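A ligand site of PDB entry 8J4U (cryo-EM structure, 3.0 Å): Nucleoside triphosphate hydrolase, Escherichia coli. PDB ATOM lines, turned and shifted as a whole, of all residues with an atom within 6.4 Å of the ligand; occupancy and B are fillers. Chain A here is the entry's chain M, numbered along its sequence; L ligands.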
ATOM      1  N   GLY A 177      18.026  -6.481  -0.244  1.00  0.00           N
ATOM      2  CA  GLY A 177      17.030  -7.279  -0.922  1.00  0.00           C
ATOM      3  C   GLY A 177      17.049  -7.235  -2.430  1.00  0.00           C
ATOM      4  O   GLY A 177      17.373  -6.218  -3.043  1.00  0.00           O
ATOM      5  N   SER A 178      16.689  -8.366  -3.042  1.00  0.00           N
ATOM      6  CA  SER A 178      16.648  -8.484  -4.483  1.00  0.00           C
ATOM      7  C   SER A 178      15.486  -7.666  -5.060  1.00  0.00           C
ATOM      8  O   SER A 178      14.749  -6.985  -4.335  1.00  0.00           O
ATOM      9  CB  SER A 178      16.541  -9.953  -4.888  1.00  0.00           C
ATOM     10  OG  SER A 178      17.810 -10.586  -4.851  1.00  0.00           O
ATOM     11  N   THR A 179      15.326  -7.735  -6.367  1.00  0.00           N
ATOM     12  CA  THR A 179      14.378  -6.909  -7.096  1.00  0.00           C
ATOM     13  C   THR A 179      12.967  -7.498  -7.038  1.00  0.00           C
ATOM     14  O   THR A 179      12.789  -8.703  -7.210  1.00  0.00           O
ATOM     15  CB  THR A 179      14.807  -6.756  -8.553  1.00  0.00           C
ATOM     16  OG1 THR A 179      16.182  -6.368  -8.604  1.00  0.00           O
ATOM     17  CG2 THR A 179      13.966  -5.725  -9.263  1.00  0.00           C
ATOM     18  N   GLY A 180      11.989  -6.621  -6.805  1.00  0.00           N
ATOM     19  CA  GLY A 180      10.606  -7.044  -6.824  1.00  0.00           C
ATOM     20  C   GLY A 180      10.088  -7.672  -5.550  1.00  0.00           C
ATOM     21  O   GLY A 180       9.130  -8.447  -5.606  1.00  0.00           O
ATOM     22  N   TYR A 181      10.710  -7.369  -4.405  1.00  0.00           N
ATOM     23  CA  TYR A 181      10.339  -8.013  -3.158  1.00  0.00           C
ATOM     24  C   TYR A 181      10.057  -7.069  -1.996  1.00  0.00           C
ATOM     25  O   TYR A 181       9.702  -7.546  -0.915  1.00  0.00           O
ATOM     26  CB  TYR A 181      11.437  -9.009  -2.729  1.00  0.00           C
ATOM     27  CG  TYR A 181      11.424 -10.282  -3.541  1.00  0.00           C
ATOM     28  CD1 TYR A 181      11.744 -10.276  -4.892  1.00  0.00           C
ATOM     29  CD2 TYR A 181      11.084 -11.497  -2.971  1.00  0.00           C
ATOM     30  CE1 TYR A 181      11.722 -11.426  -5.645  1.00  0.00           C
ATOM     31  CE2 TYR A 181      11.070 -12.655  -3.705  1.00  0.00           C
ATOM     32  CZ  TYR A 181      11.385 -12.619  -5.045  1.00  0.00           C
ATOM     33  OH  TYR A 181      11.370 -13.770  -5.792  1.00  0.00           O
ATOM     34  N   GLY A 182      10.204  -5.756  -2.170  1.00  0.00           N
ATOM     35  CA  GLY A 182       9.685  -4.813  -1.196  1.00  0.00           C
ATOM     36  C   GLY A 182      10.679  -3.900  -0.499  1.00  0.00           C
ATOM     37  O   GLY A 182      10.454  -3.523   0.648  1.00  0.00           O
ATOM     38  N   LYS A 183      11.771  -3.533  -1.175  1.00  0.00           N
ATOM     39  CA  LYS A 183      12.716  -2.606  -0.555  1.00  0.00           C
ATOM     40  C   LYS A 183      12.158  -1.188  -0.494  1.00  0.00           C
ATOM     41  O   LYS A 183      12.500  -0.436   0.431  1.00  0.00           O
ATOM     42  CB  LYS A 183      14.036  -2.598  -1.324  1.00  0.00           C
ATOM     43  CG  LYS A 183      14.938  -3.772  -1.038  1.00  0.00           C
ATOM     44  CD  LYS A 183      16.357  -3.467  -1.442  1.00  0.00           C
ATOM     45  CE  LYS A 183      16.491  -3.232  -2.941  1.00  0.00           C
ATOM     46  NZ  LYS A 183      15.822  -4.276  -3.754  1.00  0.00           N
ATOM     47  N   SER A 184      11.319  -0.804  -1.451  1.00  0.00           N
ATOM     48  CA  SER A 184      10.795   0.550  -1.523  1.00  0.00           C
ATOM     49  C   SER A 184       9.451   0.723  -0.833  1.00  0.00           C
ATOM     50  O   SER A 184       8.994   1.855  -0.673  1.00  0.00           O
ATOM     51  CB  SER A 184      10.676   0.989  -2.986  1.00  0.00           C
ATOM     52  OG  SER A 184       9.502   0.463  -3.580  1.00  0.00           O
ATOM     53  N   ASN A 185       8.815  -0.368  -0.428  1.00  0.00           N
ATOM     54  CA  ASN A 185       7.578  -0.297   0.338  1.00  0.00           C
ATOM     55  C   ASN A 185       7.819  -0.282   1.844  1.00  0.00           C
ATOM     56  O   ASN A 185       6.877  -0.084   2.609  1.00  0.00           O
ATOM     57  CB  ASN A 185       6.679  -1.478  -0.018  1.00  0.00           C
ATOM     58  CG  ASN A 185       5.283  -1.349   0.544  1.00  0.00           C
ATOM     59  OD1 ASN A 185       4.380  -0.801  -0.100  1.00  0.00           O
ATOM     60  ND2 ASN A 185       5.083  -1.870   1.746  1.00  0.00           N
ATOM     61  N   PHE A 186       9.063  -0.470   2.283  1.00  0.00           N
ATOM     62  CA  PHE A 186       9.436  -0.347   3.680  1.00  0.00           C
ATOM     63  C   PHE A 186      10.022   1.018   4.000  1.00  0.00           C
ATOM     64  O   PHE A 186       9.904   1.472   5.147  1.00  0.00           O
ATOM     65  CB  PHE A 186      10.453  -1.445   4.031  1.00  0.00           C
ATOM     66  CG  PHE A 186      11.001  -1.343   5.429  1.00  0.00           C
ATOM     67  CD1 PHE A 186      12.279  -0.866   5.642  1.00  0.00           C
ATOM     68  CD2 PHE A 186      10.245  -1.757   6.519  1.00  0.00           C
ATOM     69  CE1 PHE A 186      12.788  -0.787   6.931  1.00  0.00           C
ATOM     70  CE2 PHE A 186      10.757  -1.679   7.791  1.00  0.00           C
ATOM     71  CZ  PHE A 186      12.030  -1.187   7.997  1.00  0.00           C
ATOM     72  N   ASN A 187      10.562   1.718   3.007  1.00  0.00           N
ATOM     73  CA  ASN A 187      11.073   3.072   3.230  1.00  0.00           C
ATOM     74  C   ASN A 187       9.935   4.073   3.315  1.00  0.00           C
ATOM     75  O   ASN A 187       9.911   4.931   4.205  1.00  0.00           O
ATOM     76  CB  ASN A 187      12.033   3.462   2.110  1.00  0.00           C
ATOM     77  CG  ASN A 187      13.036   2.373   1.788  1.00  0.00           C
ATOM     78  OD1 ASN A 187      13.247   2.034   0.632  1.00  0.00           O
ATOM     79  ND2 ASN A 187      13.661   1.829   2.815  1.00  0.00           N
ATOM     80  N   ASN A 209      15.028   7.366  -9.044  1.00  0.00           N
ATOM     81  CA  ASN A 209      14.061   6.875 -10.013  1.00  0.00           C
ATOM     82  C   ASN A 209      12.768   7.676 -10.088  1.00  0.00           C
ATOM     83  O   ASN A 209      11.982   7.430 -11.007  1.00  0.00           O
ATOM     84  CB  ASN A 209      13.698   5.411  -9.706  1.00  0.00           C
ATOM     85  CG  ASN A 209      14.929   4.528  -9.549  1.00  0.00           C
ATOM     86  OD1 ASN A 209      15.526   4.469  -8.477  1.00  0.00           O
ATOM     87  ND2 ASN A 209      15.296   3.843 -10.615  1.00  0.00           N
ATOM     88  N   GLU A 211      10.189   8.156  -7.381  1.00  0.00           N
ATOM     89  CA  GLU A 211       9.239   7.237  -6.779  1.00  0.00           C
ATOM     90  C   GLU A 211       8.620   7.820  -5.505  1.00  0.00           C
ATOM     91  O   GLU A 211       7.469   7.494  -5.169  1.00  0.00           O
ATOM     92  CB  GLU A 211       9.929   5.910  -6.453  1.00  0.00           C
ATOM     93  CG  GLU A 211       9.751   4.831  -7.485  1.00  0.00           C
ATOM     94  CD  GLU A 211      10.369   3.516  -7.052  1.00  0.00           C
ATOM     95  OE1 GLU A 211      11.039   3.496  -6.007  1.00  0.00           O
ATOM     96  OE2 GLU A 211      10.187   2.506  -7.761  1.00  0.00           O
ATOM     97  N   TYR A 212       9.354   8.672  -4.805  1.00  0.00           N
ATOM     98  CA  TYR A 212       9.067   9.019  -3.421  1.00  0.00           C
ATOM     99  C   TYR A 212       8.317  10.339  -3.288  1.00  0.00           C
ATOM    100  O   TYR A 212       8.546  11.101  -2.344  1.00  0.00           O
ATOM    101  CB  TYR A 212      10.371   9.076  -2.626  1.00  0.00           C
ATOM    102  CG  TYR A 212      10.963   7.728  -2.318  1.00  0.00           C
ATOM    103  CD1 TYR A 212      10.392   6.890  -1.370  1.00  0.00           C
ATOM    104  CD2 TYR A 212      12.095   7.274  -2.986  1.00  0.00           C
ATOM    105  CE1 TYR A 212      10.939   5.664  -1.084  1.00  0.00           C
ATOM    106  CE2 TYR A 212      12.652   6.045  -2.710  1.00  0.00           C
ATOM    107  CZ  TYR A 212      12.068   5.238  -1.759  1.00  0.00           C
ATOM    108  OH  TYR A 212      12.608   4.012  -1.479  1.00  0.00           O
ATOM    109  N   GLU A 477      19.742   5.388  -1.653  1.00  0.00           N
ATOM    110  CA  GLU A 477      19.062   4.389  -2.463  1.00  0.00           C
ATOM    111  C   GLU A 477      19.947   4.038  -3.646  1.00  0.00           C
ATOM    112  O   GLU A 477      20.446   4.941  -4.331  1.00  0.00           O
ATOM    113  CB  GLU A 477      17.703   4.916  -2.935  1.00  0.00           C
ATOM    114  CG  GLU A 477      16.814   3.873  -3.573  1.00  0.00           C
ATOM    115  CD  GLU A 477      15.777   4.496  -4.488  1.00  0.00           C
ATOM    116  OE1 GLU A 477      15.464   5.684  -4.311  1.00  0.00           O
ATOM    117  OE2 GLU A 477      15.269   3.785  -5.378  1.00  0.00           O
ATOM    118  N   GLU A 478      20.147   2.745  -3.881  1.00  0.00           N
ATOM    119  CA  GLU A 478      21.039   2.259  -4.930  1.00  0.00           C
ATOM    120  C   GLU A 478      22.485   2.668  -4.628  1.00  0.00           C
ATOM    121  O   GLU A 478      23.177   3.245  -5.464  1.00  0.00           O
ATOM    122  CB  GLU A 478      20.601   2.762  -6.309  1.00  0.00           C
ATOM    123  CG  GLU A 478      19.234   2.268  -6.737  1.00  0.00           C
ATOM    124  CD  GLU A 478      19.193   0.776  -6.981  1.00  0.00           C
ATOM    125  OE1 GLU A 478      20.221   0.218  -7.409  1.00  0.00           O
ATOM    126  OE2 GLU A 478      18.135   0.163  -6.729  1.00  0.00           O
ATOM    127  N   ARG A 566       7.473 -12.600  -1.260  1.00  0.00           N
ATOM    128  CA  ARG A 566       7.274 -11.160  -1.326  1.00  0.00           C
ATOM    129  C   ARG A 566       6.667 -10.636  -0.031  1.00  0.00           C
ATOM    130  O   ARG A 566       5.754 -11.247   0.537  1.00  0.00           O
ATOM    131  CB  ARG A 566       6.379 -10.798  -2.505  1.00  0.00           C
ATOM    132  CG  ARG A 566       6.235  -9.312  -2.741  1.00  0.00           C
ATOM    133  CD  ARG A 566       5.345  -9.001  -3.918  1.00  0.00           C
ATOM    134  NE  ARG A 566       3.947  -9.333  -3.674  1.00  0.00           N
ATOM    135  CZ  ARG A 566       2.998  -9.296  -4.611  1.00  0.00           C
ATOM    136  NH1 ARG A 566       3.294  -8.948  -5.853  1.00  0.00           N
ATOM    137  NH2 ARG A 566       1.748  -9.614  -4.301  1.00  0.00           N
ATOM    138  N   GLY A 567       7.176  -9.508   0.438  1.00  0.00           N
ATOM    139  CA  GLY A 567       6.694  -8.890   1.659  1.00  0.00           C
ATOM    140  C   GLY A 567       6.891  -9.780   2.868  1.00  0.00           C
ATOM    141  O   GLY A 567       5.935 -10.096   3.584  1.00  0.00           O
ATOM    142  N   ASP A 568       8.138 -10.185   3.111  1.00  0.00           N
ATOM    143  CA  ASP A 568       8.462 -11.045   4.247  1.00  0.00           C
ATOM    144  C   ASP A 568       9.957 -10.880   4.505  1.00  0.00           C
ATOM    145  O   ASP A 568      10.769 -11.266   3.658  1.00  0.00           O
ATOM    146  CB  ASP A 568       8.096 -12.494   3.959  1.00  0.00           C
ATOM    147  CG  ASP A 568       8.219 -13.373   5.175  1.00  0.00           C
ATOM    148  OD1 ASP A 568       7.298 -13.385   6.003  1.00  0.00           O
ATOM    149  OD2 ASP A 568       9.260 -14.055   5.300  1.00  0.00           O
ATOM    150  N   SER A 583       6.219 -10.132   8.716  1.00  0.00           N
ATOM    151  CA  SER A 583       5.363  -9.934   7.559  1.00  0.00           C
ATOM    152  C   SER A 583       4.869  -8.497   7.599  1.00  0.00           C
ATOM    153  O   SER A 583       4.071  -8.134   8.472  1.00  0.00           O
ATOM    154  CB  SER A 583       4.212 -10.929   7.542  1.00  0.00           C
ATOM    155  OG  SER A 583       3.248 -10.590   6.564  1.00  0.00           O
ATOM    156  N   ILE A 584       5.336  -7.685   6.656  1.00  0.00           N
ATOM    157  CA  ILE A 584       5.154  -6.247   6.702  1.00  0.00           C
ATOM    158  C   ILE A 584       3.801  -5.872   6.114  1.00  0.00           C
ATOM    159  O   ILE A 584       3.164  -6.662   5.408  1.00  0.00           O
ATOM    160  CB  ILE A 584       6.321  -5.549   5.967  1.00  0.00           C
ATOM    161  CG1 ILE A 584       7.620  -5.777   6.724  1.00  0.00           C
ATOM    162  CG2 ILE A 584       6.073  -4.059   5.828  1.00  0.00           C
ATOM    163  CD1 ILE A 584       8.829  -5.917   5.846  1.00  0.00           C
ATOM    164  N   ASN A 585       3.343  -4.667   6.417  1.00  0.00           N
ATOM    165  CA  ASN A 585       2.072  -4.146   5.940  1.00  0.00           C
ATOM    166  C   ASN A 585       2.269  -3.231   4.743  1.00  0.00           C
ATOM    167  O   ASN A 585       3.307  -2.578   4.592  1.00  0.00           O
ATOM    168  CB  ASN A 585       1.345  -3.377   7.049  1.00  0.00           C
ATOM    169  CG  ASN A 585       1.385  -4.098   8.377  1.00  0.00           C
ATOM    170  OD1 ASN A 585       1.045  -5.283   8.468  1.00  0.00           O
ATOM    171  ND2 ASN A 585       1.799  -3.392   9.423  1.00  0.00           N
ATOM    172  N   GLN A 586       1.253  -3.184   3.878  1.00  0.00           N
ATOM    173  CA  GLN A 586       1.307  -2.354   2.687  1.00  0.00           C
ATOM    174  C   GLN A 586       1.083  -0.884   3.048  1.00  0.00           C
ATOM    175  O   GLN A 586       0.155  -0.560   3.788  1.00  0.00           O
ATOM    176  CB  GLN A 586       0.258  -2.818   1.677  1.00  0.00           C
ATOM    177  CG  GLN A 586      -0.042  -1.818   0.580  1.00  0.00           C
ATOM    178  CD  GLN A 586      -0.842  -2.430  -0.556  1.00  0.00           C
ATOM    179  OE1 GLN A 586      -0.413  -3.412  -1.161  1.00  0.00           O
ATOM    180  NE2 GLN A 586      -2.000  -1.846  -0.851  1.00  0.00           N
ATOM    181  N   PRO A 591       4.508   4.332  -3.201  1.00  0.00           N
ATOM    182  CA  PRO A 591       5.359   4.983  -4.210  1.00  0.00           C
ATOM    183  C   PRO A 591       4.733   4.979  -5.599  1.00  0.00           C
ATOM    184  O   PRO A 591       3.792   4.242  -5.858  1.00  0.00           O
ATOM    185  CB  PRO A 591       6.642   4.141  -4.176  1.00  0.00           C
ATOM    186  CG  PRO A 591       6.660   3.531  -2.837  1.00  0.00           C
ATOM    187  CD  PRO A 591       5.237   3.327  -2.414  1.00  0.00           C
HETATM  188  P1  LIG L   1      12.950  -0.896  -5.613  1.00  0.00           P
HETATM  189  S1  LIG L   1      11.553   0.080  -6.797  1.00  0.00           S
HETATM  190  O1  LIG L   1      13.825   0.194  -4.821  1.00  0.00           O
HETATM  191  O2  LIG L   1      13.839  -1.702  -6.489  1.00  0.00           O
HETATM  192  P2  LIG L   1      11.710  -3.324  -5.036  1.00  0.00           P
HETATM  193  O3  LIG L   1      11.467  -3.303  -6.520  1.00  0.00           O
HETATM  194  O4  LIG L   1      12.658  -4.337  -4.453  1.00  0.00           O
HETATM  195  O5  LIG L   1      12.196  -1.863  -4.581  1.00  0.00           O
HETATM  196  P3  LIG L   1       8.957  -2.802  -4.836  1.00  0.00           P
HETATM  197  O6  LIG L   1       8.504  -1.733  -3.870  1.00  0.00           O
HETATM  198  O7  LIG L   1       9.182  -2.459  -6.297  1.00  0.00           O
HETATM  199  O8  LIG L   1      10.295  -3.482  -4.263  1.00  0.00           O
HETATM  200  O9  LIG L   1       7.880  -4.001  -4.801  1.00  0.00           O
HETATM  201  C1  LIG L   1       7.110  -4.274  -5.961  1.00  0.00           C
HETATM  202  C2  LIG L   1       5.726  -4.793  -5.598  1.00  0.00           C
HETATM  203  O10 LIG L   1       5.760  -5.593  -4.409  1.00  0.00           O
HETATM  204  C3  LIG L   1       4.752  -3.658  -5.344  1.00  0.00           C
HETATM  205  O11 LIG L   1       3.786  -3.585  -6.390  1.00  0.00           O
HETATM  206  C4  LIG L   1       4.084  -3.976  -4.024  1.00  0.00           C
HETATM  207  O12 LIG L   1       2.661  -3.907  -4.117  1.00  0.00           O
HETATM  208  C5  LIG L   1       4.553  -5.391  -3.684  1.00  0.00           C
HETATM  209  N1  LIG L   1       4.751  -5.541  -2.231  1.00  0.00           N
HETATM  210  C6  LIG L   1       5.923  -5.479  -1.559  1.00  0.00           C
HETATM  211  N2  LIG L   1       5.720  -5.661  -0.228  1.00  0.00           N
HETATM  212  C7  LIG L   1       4.404  -5.856  -0.035  1.00  0.00           C
HETATM  213  C8  LIG L   1       3.517  -6.128   1.114  1.00  0.00           C
HETATM  214  N3  LIG L   1       4.011  -6.212   2.365  1.00  0.00           N
HETATM  215  N4  LIG L   1       2.191  -6.261   0.872  1.00  0.00           N
HETATM  216  C9  LIG L   1       1.682  -6.182  -0.363  1.00  0.00           C
HETATM  217  N5  LIG L   1       2.428  -5.938  -1.455  1.00  0.00           N
HETATM  218  C10 LIG L   1       3.769  -5.780  -1.357  1.00  0.00           C
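The side-chain amide nitrogen (ND2) of Asn 185 sits at hydrogen-bond distance from the backbone carbonyl oxygen (O) of Asn 585 (3.4 Å). N of Gly 567 is in hydrogen-bond range of O of Tyr 181. The side-chain amino group (NZ) of Lys 183 sits at hydrogen-bond distance from the backbone carbonyl oxygen (O) of Ser 178 (3.0 Å). OD1 of Asn 209 lies close to OE2 of Glu 477. The side-chain amino group (NZ) of Lys 183 sits at hydrogen-bond distance from the backbone carbonyl oxygen (O) of Gly 177 (2.6 Å). The backbone carbonyl oxygen (O) of Lys 183 sits close to the side-chain amide oxygen (OD1) of Asn 187.
O of Ser 178 lies close to O4 of the ligand, at 3.4 Å. A sulfur (S1) of the ligand lies close to the side-chain carboxylate of Glu 211 (2.9 Å). Merely in contact with the ligand: Arg 566 (3.5 Å), Gln 586 (3.6 Å), Tyr 181 (3.6 Å), Asn 185 (3.7 Å), Gly 567 (3.9 Å) and Glu 477 (3.9 Å). Within 4 Å of the ligand: Ser 178, Gly 180, Tyr 181, Gly 182, Lys 183, Ser 184, Asn 185, Glu 211, Glu 477, Arg 566, Gly 567, Ile 584 and Gln 586.
N of Lys 183 sits at hydrogen-bond distance from O8 of the ligand (3.4 Å). O5 of the ligand lies within hydrogen-bond range of N of Ser 184, 3.4 Å away. N of Gly 182 lies within hydrogen-bond range of O8 of the ligand, 3.1 Å away. The backbone carbonyl oxygen (O) of Ile 584 lies within hydrogen-bond range of a nitrogen (N3) of the ligand, at 3.2 Å. The side-chain hydroxyl (OG) of Ser 184 is in hydrogen-bond range of an oxygen (O6) of the ligand (2.4 Å). An oxygen (O4) of the ligand lies within hydrogen-bond range of the backbone NH (N) of Gly 180. An oxygen (O4) of the ligand lies within salt-bridge range of the side-chain amino group (NZ) of Lys 183, at 3.2 Å.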
